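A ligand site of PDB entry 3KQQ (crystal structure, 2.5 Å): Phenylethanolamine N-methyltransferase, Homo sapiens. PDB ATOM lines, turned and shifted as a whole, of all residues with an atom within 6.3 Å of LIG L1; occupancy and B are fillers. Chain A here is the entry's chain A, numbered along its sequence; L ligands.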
ATOM      1  N   ALA A  24       0.812 -20.421   3.945  1.00  0.00           N
ATOM      2  CA  ALA A  24      -0.158 -21.316   3.339  1.00  0.00           C
ATOM      3  C   ALA A  24       0.220 -22.789   3.533  1.00  0.00           C
ATOM      4  O   ALA A  24      -0.629 -23.609   3.880  1.00  0.00           O
ATOM      5  CB  ALA A  24      -0.317 -21.004   1.848  1.00  0.00           C
ATOM      6  N   TYR A  27      -0.840 -25.058   6.582  1.00  0.00           N
ATOM      7  CA  TYR A  27      -2.068 -25.843   6.674  1.00  0.00           C
ATOM      8  C   TYR A  27      -1.826 -27.268   6.233  1.00  0.00           C
ATOM      9  O   TYR A  27      -2.706 -28.109   6.355  1.00  0.00           O
ATOM     10  CB  TYR A  27      -3.217 -25.200   5.902  1.00  0.00           C
ATOM     11  CG  TYR A  27      -3.972 -24.195   6.739  1.00  0.00           C
ATOM     12  CD1 TYR A  27      -3.738 -22.820   6.595  1.00  0.00           C
ATOM     13  CD2 TYR A  27      -4.875 -24.610   7.703  1.00  0.00           C
ATOM     14  CE1 TYR A  27      -4.413 -21.905   7.369  1.00  0.00           C
ATOM     15  CE2 TYR A  27      -5.556 -23.700   8.483  1.00  0.00           C
ATOM     16  CZ  TYR A  27      -5.318 -22.354   8.317  1.00  0.00           C
ATOM     17  OH  TYR A  27      -5.994 -21.456   9.090  1.00  0.00           O
ATOM     18  N   PHE A  30      -1.775 -29.342   9.306  1.00  0.00           N
ATOM     19  CA  PHE A  30      -3.023 -29.198  10.060  1.00  0.00           C
ATOM     20  C   PHE A  30      -3.657 -30.546  10.437  1.00  0.00           C
ATOM     21  O   PHE A  30      -4.049 -31.321   9.559  1.00  0.00           O
ATOM     22  CB  PHE A  30      -3.998 -28.355   9.242  1.00  0.00           C
ATOM     23  CG  PHE A  30      -5.336 -28.153   9.883  1.00  0.00           C
ATOM     24  CD1 PHE A  30      -5.684 -26.921  10.414  1.00  0.00           C
ATOM     25  CD2 PHE A  30      -6.277 -29.191   9.917  1.00  0.00           C
ATOM     26  CE1 PHE A  30      -6.930 -26.724  10.995  1.00  0.00           C
ATOM     27  CE2 PHE A  30      -7.509 -28.995  10.494  1.00  0.00           C
ATOM     28  CZ  PHE A  30      -7.847 -27.765  11.034  1.00  0.00           C
ATOM     29  N   TYR A  35      -7.423 -30.226  16.070  1.00  0.00           N
ATOM     30  CA  TYR A  35      -8.224 -29.013  15.961  1.00  0.00           C
ATOM     31  C   TYR A  35      -9.561 -29.188  16.676  1.00  0.00           C
ATOM     32  O   TYR A  35      -9.980 -28.314  17.446  1.00  0.00           O
ATOM     33  CB  TYR A  35      -8.435 -28.602  14.504  1.00  0.00           C
ATOM     34  CG  TYR A  35      -9.344 -27.400  14.321  1.00  0.00           C
ATOM     35  CD1 TYR A  35      -8.851 -26.094  14.376  1.00  0.00           C
ATOM     36  CD2 TYR A  35     -10.721 -27.566  14.073  1.00  0.00           C
ATOM     37  CE1 TYR A  35      -9.687 -25.002  14.206  1.00  0.00           C
ATOM     38  CE2 TYR A  35     -11.556 -26.475  13.903  1.00  0.00           C
ATOM     39  CZ  TYR A  35     -11.040 -25.201  13.970  1.00  0.00           C
ATOM     40  OH  TYR A  35     -11.863 -24.111  13.796  1.00  0.00           O
ATOM     41  N   ASN A  39     -10.833 -27.185  20.218  1.00  0.00           N
ATOM     42  CA  ASN A  39     -11.919 -26.227  20.021  1.00  0.00           C
ATOM     43  C   ASN A  39     -13.318 -26.741  20.312  1.00  0.00           C
ATOM     44  O   ASN A  39     -14.204 -25.951  20.627  1.00  0.00           O
ATOM     45  CB  ASN A  39     -11.858 -25.657  18.604  1.00  0.00           C
ATOM     46  CG  ASN A  39     -10.609 -24.821  18.373  1.00  0.00           C
ATOM     47  OD1 ASN A  39     -10.376 -23.829  19.054  1.00  0.00           O
ATOM     48  ND2 ASN A  39      -9.809 -25.226  17.403  1.00  0.00           N
ATOM     49  N   TYR A  40     -13.528 -28.055  20.210  1.00  0.00           N
ATOM     50  CA  TYR A  40     -14.887 -28.591  20.336  1.00  0.00           C
ATOM     51  C   TYR A  40     -15.044 -29.685  21.384  1.00  0.00           C
ATOM     52  O   TYR A  40     -16.112 -30.267  21.521  1.00  0.00           O
ATOM     53  CB  TYR A  40     -15.434 -28.977  18.953  1.00  0.00           C
ATOM     54  CG  TYR A  40     -15.501 -27.748  18.061  1.00  0.00           C
ATOM     55  CD1 TYR A  40     -14.417 -27.389  17.259  1.00  0.00           C
ATOM     56  CD2 TYR A  40     -16.608 -26.909  18.097  1.00  0.00           C
ATOM     57  CE1 TYR A  40     -14.463 -26.249  16.464  1.00  0.00           C
ATOM     58  CE2 TYR A  40     -16.657 -25.769  17.317  1.00  0.00           C
ATOM     59  CZ  TYR A  40     -15.584 -25.437  16.511  1.00  0.00           C
ATOM     60  OH  TYR A  40     -15.640 -24.303  15.736  1.00  0.00           O
ATOM     61  N   LYS A  57     -22.290 -19.176  20.031  1.00  0.00           N
ATOM     62  CA  LYS A  57     -22.353 -19.364  18.589  1.00  0.00           C
ATOM     63  C   LYS A  57     -23.663 -20.014  18.131  1.00  0.00           C
ATOM     64  O   LYS A  57     -24.333 -19.512  17.228  1.00  0.00           O
ATOM     65  CB  LYS A  57     -21.162 -20.178  18.116  1.00  0.00           C
ATOM     66  CG  LYS A  57     -19.845 -19.439  18.267  1.00  0.00           C
ATOM     67  CD  LYS A  57     -18.707 -20.189  17.588  1.00  0.00           C
ATOM     68  CE  LYS A  57     -18.514 -21.585  18.171  1.00  0.00           C
ATOM     69  NZ  LYS A  57     -17.308 -22.203  17.582  1.00  0.00           N
ATOM     70  N   ASP A  77     -21.259 -23.549   2.749  1.00  0.00           N
ATOM     71  CA  ASP A  77     -20.456 -23.330   3.945  1.00  0.00           C
ATOM     72  C   ASP A  77     -18.985 -23.245   3.532  1.00  0.00           C
ATOM     73  O   ASP A  77     -18.394 -24.247   3.108  1.00  0.00           O
ATOM     74  CB  ASP A  77     -20.675 -24.483   4.943  1.00  0.00           C
ATOM     75  CG  ASP A  77     -19.911 -24.298   6.238  1.00  0.00           C
ATOM     76  OD1 ASP A  77     -19.604 -23.149   6.605  1.00  0.00           O
ATOM     77  OD2 ASP A  77     -19.621 -25.314   6.906  1.00  0.00           O
ATOM     78  N   ILE A  78     -18.427 -22.045   3.664  1.00  0.00           N
ATOM     79  CA  ILE A  78     -17.055 -21.760   3.241  1.00  0.00           C
ATOM     80  C   ILE A  78     -16.060 -22.139   4.309  1.00  0.00           C
ATOM     81  O   ILE A  78     -16.134 -21.633   5.445  1.00  0.00           O
ATOM     82  CB  ILE A  78     -16.858 -20.242   2.997  1.00  0.00           C
ATOM     83  CG1 ILE A  78     -18.032 -19.641   2.211  1.00  0.00           C
ATOM     84  CG2 ILE A  78     -15.514 -19.994   2.321  1.00  0.00           C
ATOM     85  CD1 ILE A  78     -18.277 -20.279   0.839  1.00  0.00           C
ATOM     86  N   GLY A  79     -15.110 -23.013   3.972  1.00  0.00           N
ATOM     87  CA  GLY A  79     -14.092 -23.454   4.907  1.00  0.00           C
ATOM     88  C   GLY A  79     -14.644 -24.163   6.137  1.00  0.00           C
ATOM     89  O   GLY A  79     -14.427 -23.720   7.268  1.00  0.00           O
ATOM     90  N   SER A  80     -15.344 -25.269   5.903  1.00  0.00           N
ATOM     91  CA  SER A  80     -16.059 -26.012   6.945  1.00  0.00           C
ATOM     92  C   SER A  80     -15.144 -26.657   7.963  1.00  0.00           C
ATOM     93  O   SER A  80     -15.559 -26.951   9.114  1.00  0.00           O
ATOM     94  CB  SER A  80     -16.891 -27.109   6.286  1.00  0.00           C
ATOM     95  OG  SER A  80     -17.840 -26.575   5.388  1.00  0.00           O
ATOM     96  N   GLY A  81     -13.901 -26.910   7.554  1.00  0.00           N
ATOM     97  CA  GLY A  81     -13.017 -27.755   8.324  1.00  0.00           C
ATOM     98  C   GLY A  81     -13.653 -29.105   8.628  1.00  0.00           C
ATOM     99  O   GLY A  81     -14.410 -29.646   7.827  1.00  0.00           O
ATOM    100  N   PRO A  82     -13.347 -29.651   9.806  1.00  0.00           N
ATOM    101  CA  PRO A  82     -13.924 -30.937  10.197  1.00  0.00           C
ATOM    102  C   PRO A  82     -15.192 -30.729  11.005  1.00  0.00           C
ATOM    103  O   PRO A  82     -15.562 -31.627  11.743  1.00  0.00           O
ATOM    104  CB  PRO A  82     -12.858 -31.517  11.125  1.00  0.00           C
ATOM    105  CG  PRO A  82     -11.954 -30.342  11.520  1.00  0.00           C
ATOM    106  CD  PRO A  82     -12.477 -29.101  10.856  1.00  0.00           C
ATOM    107  N   THR A  83     -15.829 -29.563  10.909  1.00  0.00           N
ATOM    108  CA  THR A  83     -16.935 -29.270  11.811  1.00  0.00           C
ATOM    109  C   THR A  83     -18.291 -29.132  11.102  1.00  0.00           C
ATOM    110  O   THR A  83     -18.353 -28.755   9.930  1.00  0.00           O
ATOM    111  CB  THR A  83     -16.627 -28.061  12.750  1.00  0.00           C
ATOM    112  OG1 THR A  83     -16.880 -26.817  12.087  1.00  0.00           O
ATOM    113  CG2 THR A  83     -15.192 -28.118  13.239  1.00  0.00           C
ATOM    114  N   TYR A  85     -21.262 -28.102  13.236  1.00  0.00           N
ATOM    115  CA  TYR A  85     -22.148 -27.387  14.171  1.00  0.00           C
ATOM    116  C   TYR A  85     -22.779 -26.167  13.526  1.00  0.00           C
ATOM    117  O   TYR A  85     -23.902 -25.777  13.863  1.00  0.00           O
ATOM    118  CB  TYR A  85     -21.396 -26.947  15.424  1.00  0.00           C
ATOM    119  CG  TYR A  85     -20.421 -25.804  15.161  1.00  0.00           C
ATOM    120  CD1 TYR A  85     -20.770 -24.491  15.454  1.00  0.00           C
ATOM    121  CD2 TYR A  85     -19.168 -26.045  14.616  1.00  0.00           C
ATOM    122  CE1 TYR A  85     -19.895 -23.451  15.196  1.00  0.00           C
ATOM    123  CE2 TYR A  85     -18.285 -25.024  14.367  1.00  0.00           C
ATOM    124  CZ  TYR A  85     -18.657 -23.720  14.663  1.00  0.00           C
ATOM    125  OH  TYR A  85     -17.784 -22.697  14.404  1.00  0.00           O
ATOM    126  N   GLN A  86     -22.060 -25.559  12.591  1.00  0.00           N
ATOM    127  CA  GLN A  86     -22.473 -24.290  12.002  1.00  0.00           C
ATOM    128  C   GLN A  86     -23.603 -24.432  10.990  1.00  0.00           C
ATOM    129  O   GLN A  86     -23.996 -23.439  10.379  1.00  0.00           O
ATOM    130  CB  GLN A  86     -21.272 -23.558  11.368  1.00  0.00           C
ATOM    131  CG  GLN A  86     -20.640 -24.231  10.148  1.00  0.00           C
ATOM    132  CD  GLN A  86     -19.608 -25.283  10.512  1.00  0.00           C
ATOM    133  OE1 GLN A  86     -19.608 -25.824  11.625  1.00  0.00           O
ATOM    134  NE2 GLN A  86     -18.716 -25.573   9.571  1.00  0.00           N
ATOM    135  N   ASP A 101     -13.948 -27.268   2.033  1.00  0.00           N
ATOM    136  CA  ASP A 101     -12.709 -26.963   2.724  1.00  0.00           C
ATOM    137  C   ASP A 101     -11.528 -27.113   1.790  1.00  0.00           C
ATOM    138  O   ASP A 101     -11.620 -27.770   0.754  1.00  0.00           O
ATOM    139  CB  ASP A 101     -12.493 -27.837   3.958  1.00  0.00           C
ATOM    140  CG  ASP A 101     -11.461 -27.247   4.891  1.00  0.00           C
ATOM    141  OD1 ASP A 101     -11.742 -26.179   5.484  1.00  0.00           O
ATOM    142  OD2 ASP A 101     -10.371 -27.848   5.036  1.00  0.00           O
ATOM    143  N   PHE A 102     -10.418 -26.496   2.176  1.00  0.00           N
ATOM    144  CA  PHE A 102      -9.204 -26.464   1.389  1.00  0.00           C
ATOM    145  C   PHE A 102      -8.411 -27.765   1.531  1.00  0.00           C
ATOM    146  O   PHE A 102      -7.748 -28.204   0.589  1.00  0.00           O
ATOM    147  CB  PHE A 102      -8.359 -25.258   1.800  1.00  0.00           C
ATOM    148  CG  PHE A 102      -7.039 -25.170   1.109  1.00  0.00           C
ATOM    149  CD1 PHE A 102      -6.942 -24.634  -0.164  1.00  0.00           C
ATOM    150  CD2 PHE A 102      -5.882 -25.603   1.734  1.00  0.00           C
ATOM    151  CE1 PHE A 102      -5.718 -24.535  -0.810  1.00  0.00           C
ATOM    152  CE2 PHE A 102      -4.651 -25.510   1.089  1.00  0.00           C
ATOM    153  CZ  PHE A 102      -4.568 -24.973  -0.179  1.00  0.00           C
ATOM    154  N   LEU A 103      -8.491 -28.391   2.704  1.00  0.00           N
ATOM    155  CA  LEU A 103      -7.748 -29.632   2.967  1.00  0.00           C
ATOM    156  C   LEU A 103      -8.538 -30.923   2.711  1.00  0.00           C
ATOM    157  O   LEU A 103      -9.696 -31.062   3.118  1.00  0.00           O
ATOM    158  CB  LEU A 103      -7.217 -29.643   4.405  1.00  0.00           C
ATOM    159  CG  LEU A 103      -6.126 -28.639   4.794  1.00  0.00           C
ATOM    160  CD1 LEU A 103      -6.049 -28.492   6.317  1.00  0.00           C
ATOM    161  CD2 LEU A 103      -4.769 -29.027   4.211  1.00  0.00           C
ATOM    162  N   ASN A 106      -9.641 -32.695   6.127  1.00  0.00           N
ATOM    163  CA  ASN A 106     -10.897 -32.172   6.647  1.00  0.00           C
ATOM    164  C   ASN A 106     -12.112 -32.735   5.920  1.00  0.00           C
ATOM    165  O   ASN A 106     -13.073 -33.174   6.560  1.00  0.00           O
ATOM    166  CB  ASN A 106     -10.914 -30.649   6.574  1.00  0.00           C
ATOM    167  CG  ASN A 106     -10.215 -30.018   7.754  1.00  0.00           C
ATOM    168  OD1 ASN A 106      -9.728 -28.892   7.675  1.00  0.00           O
ATOM    169  ND2 ASN A 106     -10.158 -30.748   8.861  1.00  0.00           N
ATOM    170  N   ILE A 157     -11.915 -26.005  -2.102  1.00  0.00           N
ATOM    171  CA  ILE A 157     -12.171 -24.582  -2.228  1.00  0.00           C
ATOM    172  C   ILE A 157     -10.942 -23.798  -1.771  1.00  0.00           C
ATOM    173  O   ILE A 157     -10.227 -24.219  -0.849  1.00  0.00           O
ATOM    174  CB  ILE A 157     -13.420 -24.178  -1.413  1.00  0.00           C
ATOM    175  CG1 ILE A 157     -13.775 -22.706  -1.653  1.00  0.00           C
ATOM    176  CG2 ILE A 157     -13.224 -24.479   0.093  1.00  0.00           C
ATOM    177  CD1 ILE A 157     -15.114 -22.290  -1.096  1.00  0.00           C
ATOM    178  N   ASP A 158     -10.670 -22.679  -2.432  1.00  0.00           N
ATOM    179  CA  ASP A 158      -9.583 -21.780  -2.039  1.00  0.00           C
ATOM    180  C   ASP A 158     -10.027 -20.347  -2.169  1.00  0.00           C
ATOM    181  O   ASP A 158     -10.133 -19.815  -3.283  1.00  0.00           O
ATOM    182  CB  ASP A 158      -8.344 -21.987  -2.911  1.00  0.00           C
ATOM    183  CG  ASP A 158      -7.209 -21.065  -2.514  1.00  0.00           C
ATOM    184  OD1 ASP A 158      -7.472 -19.994  -1.917  1.00  0.00           O
ATOM    185  OD2 ASP A 158      -6.037 -21.407  -2.789  1.00  0.00           O
ATOM    186  N   VAL A 159     -10.255 -19.709  -1.028  1.00  0.00           N
ATOM    187  CA  VAL A 159     -10.827 -18.364  -1.014  1.00  0.00           C
ATOM    188  C   VAL A 159      -9.902 -17.320  -1.644  1.00  0.00           C
ATOM    189  O   VAL A 159     -10.368 -16.266  -2.089  1.00  0.00           O
ATOM    190  CB  VAL A 159     -11.215 -17.950   0.407  1.00  0.00           C
ATOM    191  CG1 VAL A 159     -12.314 -18.878   0.922  1.00  0.00           C
ATOM    192  CG2 VAL A 159      -9.997 -17.997   1.326  1.00  0.00           C
ATOM    193  N   HIS A 160      -8.610 -17.612  -1.711  1.00  0.00           N
ATOM    194  CA  HIS A 160      -7.674 -16.702  -2.349  1.00  0.00           C
ATOM    195  C   HIS A 160      -7.952 -16.543  -3.845  1.00  0.00           C
ATOM    196  O   HIS A 160      -7.663 -15.506  -4.425  1.00  0.00           O
ATOM    197  CB  HIS A 160      -6.246 -17.150  -2.099  1.00  0.00           C
ATOM    198  CG  HIS A 160      -5.884 -17.220  -0.655  1.00  0.00           C
ATOM    199  ND1 HIS A 160      -6.204 -16.207   0.225  1.00  0.00           N
ATOM    200  CD2 HIS A 160      -5.260 -18.168   0.071  1.00  0.00           C
ATOM    201  CE1 HIS A 160      -5.780 -16.537   1.432  1.00  0.00           C
ATOM    202  NE2 HIS A 160      -5.199 -17.722   1.365  1.00  0.00           N
ATOM    203  N   SER A 180     -19.886 -19.068   6.885  1.00  0.00           N
ATOM    204  CA  SER A 180     -18.470 -19.342   7.055  1.00  0.00           C
ATOM    205  C   SER A 180     -18.047 -18.992   8.461  1.00  0.00           C
ATOM    206  O   SER A 180     -18.377 -17.908   8.965  1.00  0.00           O
ATOM    207  CB  SER A 180     -17.616 -18.562   6.058  1.00  0.00           C
ATOM    208  OG  SER A 180     -16.241 -18.860   6.248  1.00  0.00           O
ATOM    209  N   ALA A 181     -17.301 -19.894   9.085  1.00  0.00           N
ATOM    210  CA  ALA A 181     -16.863 -19.696  10.455  1.00  0.00           C
ATOM    211  C   ALA A 181     -15.370 -19.958  10.649  1.00  0.00           C
ATOM    212  O   ALA A 181     -14.886 -21.057  10.367  1.00  0.00           O
ATOM    213  CB  ALA A 181     -17.694 -20.564  11.398  1.00  0.00           C
ATOM    214  N   PHE A 182     -14.661 -18.947  11.151  1.00  0.00           N
ATOM    215  CA  PHE A 182     -13.257 -19.089  11.530  1.00  0.00           C
ATOM    216  C   PHE A 182     -12.359 -19.479  10.350  1.00  0.00           C
ATOM    217  O   PHE A 182     -11.323 -20.120  10.504  1.00  0.00           O
ATOM    218  CB  PHE A 182     -13.109 -20.095  12.674  1.00  0.00           C
ATOM    219  CG  PHE A 182     -13.928 -19.734  13.878  1.00  0.00           C
ATOM    220  CD1 PHE A 182     -15.144 -20.359  14.127  1.00  0.00           C
ATOM    221  CD2 PHE A 182     -13.492 -18.738  14.762  1.00  0.00           C
ATOM    222  CE1 PHE A 182     -15.900 -20.026  15.236  1.00  0.00           C
ATOM    223  CE2 PHE A 182     -14.238 -18.394  15.873  1.00  0.00           C
ATOM    224  CZ  PHE A 182     -15.444 -19.038  16.117  1.00  0.00           C
ATOM    225  N   CYS A 183     -12.774 -19.064   9.160  1.00  0.00           N
ATOM    226  CA  CYS A 183     -12.020 -19.359   7.965  1.00  0.00           C
ATOM    227  C   CYS A 183     -11.154 -18.180   7.512  1.00  0.00           C
ATOM    228  O   CYS A 183      -9.937 -18.202   7.644  1.00  0.00           O
ATOM    229  CB  CYS A 183     -12.972 -19.788   6.849  1.00  0.00           C
ATOM    230  SG  CYS A 183     -12.140 -20.189   5.315  1.00  0.00           S
ATOM    231  N   LEU A 184     -11.799 -17.139   6.985  1.00  0.00           N
ATOM    232  CA  LEU A 184     -11.098 -16.039   6.337  1.00  0.00           C
ATOM    233  C   LEU A 184      -9.914 -15.480   7.128  1.00  0.00           C
ATOM    234  O   LEU A 184      -8.778 -15.481   6.642  1.00  0.00           O
ATOM    235  CB  LEU A 184     -12.057 -14.910   5.982  1.00  0.00           C
ATOM    236  CG  LEU A 184     -13.259 -15.348   5.159  1.00  0.00           C
ATOM    237  CD1 LEU A 184     -13.935 -14.136   4.563  1.00  0.00           C
ATOM    238  CD2 LEU A 184     -12.823 -16.315   4.066  1.00  0.00           C
ATOM    239  N   ALA A 186      -8.312 -16.674   9.371  1.00  0.00           N
ATOM    240  CA  ALA A 186      -7.361 -17.735   9.674  1.00  0.00           C
ATOM    241  C   ALA A 186      -6.556 -18.158   8.451  1.00  0.00           C
ATOM    242  O   ALA A 186      -5.547 -18.863   8.570  1.00  0.00           O
ATOM    243  CB  ALA A 186      -8.090 -18.946  10.279  1.00  0.00           C
ATOM    244  N   VAL A 187      -7.001 -17.744   7.263  1.00  0.00           N
ATOM    245  CA  VAL A 187      -6.253 -18.049   6.052  1.00  0.00           C
ATOM    246  C   VAL A 187      -5.626 -16.800   5.440  1.00  0.00           C
ATOM    247  O   VAL A 187      -5.126 -16.818   4.325  1.00  0.00           O
ATOM    248  CB  VAL A 187      -7.130 -18.766   4.998  1.00  0.00           C
ATOM    249  CG1 VAL A 187      -7.726 -20.046   5.579  1.00  0.00           C
ATOM    250  CG2 VAL A 187      -8.235 -17.832   4.500  1.00  0.00           C
ATOM    251  N   TYR A 222      -3.070 -19.921  16.175  1.00  0.00           N
ATOM    252  CA  TYR A 222      -3.703 -21.027  16.874  1.00  0.00           C
ATOM    253  C   TYR A 222      -3.048 -22.329  16.437  1.00  0.00           C
ATOM    254  O   TYR A 222      -2.482 -22.421  15.342  1.00  0.00           O
ATOM    255  CB  TYR A 222      -5.207 -21.065  16.623  1.00  0.00           C
ATOM    256  CG  TYR A 222      -5.602 -21.541  15.235  1.00  0.00           C
ATOM    257  CD1 TYR A 222      -6.002 -22.854  15.034  1.00  0.00           C
ATOM    258  CD2 TYR A 222      -5.587 -20.676  14.138  1.00  0.00           C
ATOM    259  CE1 TYR A 222      -6.389 -23.309  13.779  1.00  0.00           C
ATOM    260  CE2 TYR A 222      -5.961 -21.121  12.872  1.00  0.00           C
ATOM    261  CZ  TYR A 222      -6.366 -22.446  12.705  1.00  0.00           C
ATOM    262  OH  TYR A 222      -6.748 -22.908  11.465  1.00  0.00           O
HETATM  263  N1  LIG L   1     -15.379 -23.916   9.824  1.00  0.00           N
HETATM  264  C1  LIG L   1     -14.559 -24.458  10.903  1.00  0.00           C
HETATM  265  C2  LIG L   1     -13.271 -23.625  10.882  1.00  0.00           C
HETATM  266  C3  LIG L   1     -12.107 -24.462  10.360  1.00  0.00           C
HETATM  267  S1  LIG L   1     -10.609 -23.515  10.755  1.00  0.00           S
HETATM  268  C4  LIG L   1     -15.219 -24.161  12.270  1.00  0.00           C
HETATM  269  O1  LIG L   1     -16.113 -23.382  12.358  1.00  0.00           O
HETATM  270  O2  LIG L   1     -14.443 -24.373  13.410  1.00  0.00           O
HETATM  271  C5  LIG L   1      -9.999 -22.718   9.235  1.00  0.00           C
HETATM  272  C6  LIG L   1     -10.330 -23.602   8.014  1.00  0.00           C
HETATM  273  O3  LIG L   1      -9.930 -22.902   6.802  1.00  0.00           O
HETATM  274  C7  LIG L   1      -9.577 -24.944   8.024  1.00  0.00           C
HETATM  275  O4  LIG L   1     -10.473 -26.028   7.894  1.00  0.00           O
HETATM  276  C8  LIG L   1      -8.683 -24.820   6.822  1.00  0.00           C
HETATM  277  O5  LIG L   1      -8.214 -26.020   6.260  1.00  0.00           O
HETATM  278  C9  LIG L   1      -9.493 -23.947   5.881  1.00  0.00           C
HETATM  279  N2  LIG L   1      -8.606 -23.365   4.895  1.00  0.00           N
HETATM  280  C10 LIG L   1      -7.114 -23.318   4.971  1.00  0.00           C
HETATM  281  N3  LIG L   1      -6.628 -22.607   3.792  1.00  0.00           N
HETATM  282  C11 LIG L   1      -7.793 -22.201   3.013  1.00  0.00           C
HETATM  283  C12 LIG L   1      -7.910 -21.454   1.719  1.00  0.00           C
HETATM  284  N4  LIG L   1      -6.694 -21.002   1.055  1.00  0.00           N
HETATM  285  N5  LIG L   1      -9.233 -21.181   1.150  1.00  0.00           N
HETATM  286  C13 LIG L   1     -10.480 -21.659   1.843  1.00  0.00           C
HETATM  287  N6  LIG L   1     -10.363 -22.422   3.122  1.00  0.00           N
HETATM  288  C14 LIG L   1      -9.028 -22.668   3.694  1.00  0.00           C
HETATM  289  O1  LG2 L   2     -12.568 -22.578  15.817  1.00  0.00           O
HETATM  290  C1  LG2 L   2     -12.165 -21.600  16.426  1.00  0.00           C
HETATM  291  O2  LG2 L   2     -11.010 -21.017  16.142  1.00  0.00           O
HETATM  292  C2  LG2 L   2     -13.017 -21.026  17.562  1.00  0.00           C
HETATM  293  C3  LG2 L   2     -14.294 -21.502  17.778  1.00  0.00           C
HETATM  294  C4  LG2 L   2     -15.050 -20.966  18.811  1.00  0.00           C
HETATM  295  C5  LG2 L   2     -14.510 -19.952  19.616  1.00  0.00           C
HETATM  296  N1  LG2 L   2     -13.263 -19.495  19.385  1.00  0.00           N
HETATM  297  C6  LG2 L   2     -12.505 -20.009  18.376  1.00  0.00           C
HETATM  298  O3  LG2 L   2     -11.225 -19.528  18.167  1.00  0.00           O
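The side-chain hydroxyl (OH) of Tyr 40 sits at hydrogen-bond distance from an oxygen (O2) of LIG L1, at 2.6 Å.
An oxygen (O2) of LIG L1 sits at hydrogen-bond distance from the side-chain hydroxyl of Tyr 35, 2.6 Å away.
An oxygen (O4) of LIG L1 is in hydrogen-bond range of the side-chain carboxylate (OD1) of Asp 101 (2.7 Å).
The side-chain hydroxyl of Tyr 85 is in hydrogen-bond range of an oxygen (O1) of LIG L1 (2.7 Å).
O of Gly 79 lies within hydrogen-bond range of N1 of LIG L1.
A nitrogen (N5) of LIG L1 is in hydrogen-bond range of the backbone NH of Val 159, at 2.8 Å.
O of Ala 181 is in hydrogen-bond range of N1 of LIG L1 (3.0 Å).
OD1 of Asn 106 lies within hydrogen-bond range of O4 of LIG L1, at 3.0 Å.
A nitrogen (N1) of LIG L1 sits at hydrogen-bond distance from the backbone carbonyl oxygen (O) of Ser 80 (3.1 Å).
A nitrogen (N4) of LIG L1 lies within hydrogen-bond range of the side-chain carboxylate (OD1) of Asp 158 (3.2 Å).
N6 of LIG L1 lies within hydrogen-bond range of SG of Cys 183, 3.6 Å away.
The side-chain hydroxyl of Tyr 35 is in hydrogen-bond range of an oxygen (O1) of LG2 L2.
The side-chain hydroxyl (OH) of Tyr 40 sits at hydrogen-bond distance from the side-chain amino group (NZ) of Lys 57 (3.3 Å).
The side-chain amide oxygen (OD1) of Asn 106 lies close to the side-chain carboxylate (OD2) of Asp 101 (2.9 Å).
OD2 of Asp 101 lies within hydrogen-bond range of N of Leu 103.
OG1 of Thr 83 lies within hydrogen-bond range of O of Ser 80.
The side-chain hydroxyl of Thr 83 lies within hydrogen-bond range of the side-chain amide oxygen of Gln 86, at 2.9 Å.
The side-chain carboxylate (OD1) of Asp 158 lies within hydrogen-bond range of the backbone NH (N) of His 160, at 2.6 Å.
OH of Tyr 27 sits at hydrogen-bond distance from OH of Tyr 222.
NE2 of Gln 86 sits at hydrogen-bond distance from OD2 of Asp 77, 2.8 Å away.
A sulfur (S1) of LIG L1 lies close to the backbone carbonyl oxygen (O) of Phe 182, at 3.5 Å.
Tyr 27 touches LIG L1.
Gly 81 touches LIG L1 (CA to O4, 3.1 Å).
Thr 83 touches LIG L1 (OG1 to C4, 3.1 Å).
Gln 86 touches LIG L1 (NE2 to N1, 3.7 Å).
Phe 102 touches LIG L1.
CD1 of Leu 103 touches O5 of LIG L1 (3.3 Å).
Ile 157 touches LIG L1.
His 160 touches LIG L1.
Val 187 touches LIG L1.
Tyr 222 touches LIG L1 (OH to C5, 3.9 Å).
Hydrophobic or aromatic side chains within 4 Å of LIG L1: Tyr 27, Tyr 35, Tyr 40, Tyr 85, Phe 102, Leu 103, Val 159, His 160, Ala 181, Phe 182 and Val 187.
Within 4 Å of LIG L1: Tyr 27, Tyr 35, Tyr 40, Gly 79, Ser 80, Gly 81, Thr 83, Tyr 85, Gln 86, Asp 101, Phe 102, Leu 103, Asn 106, Ile 157, Asp 158, Val 159, His 160, Ala 181, Phe 182, Cys 183, Val 187 and Tyr 222.
The nearest printed residue that does not touch LIG L1 is Ala 186 (4.4 Å).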
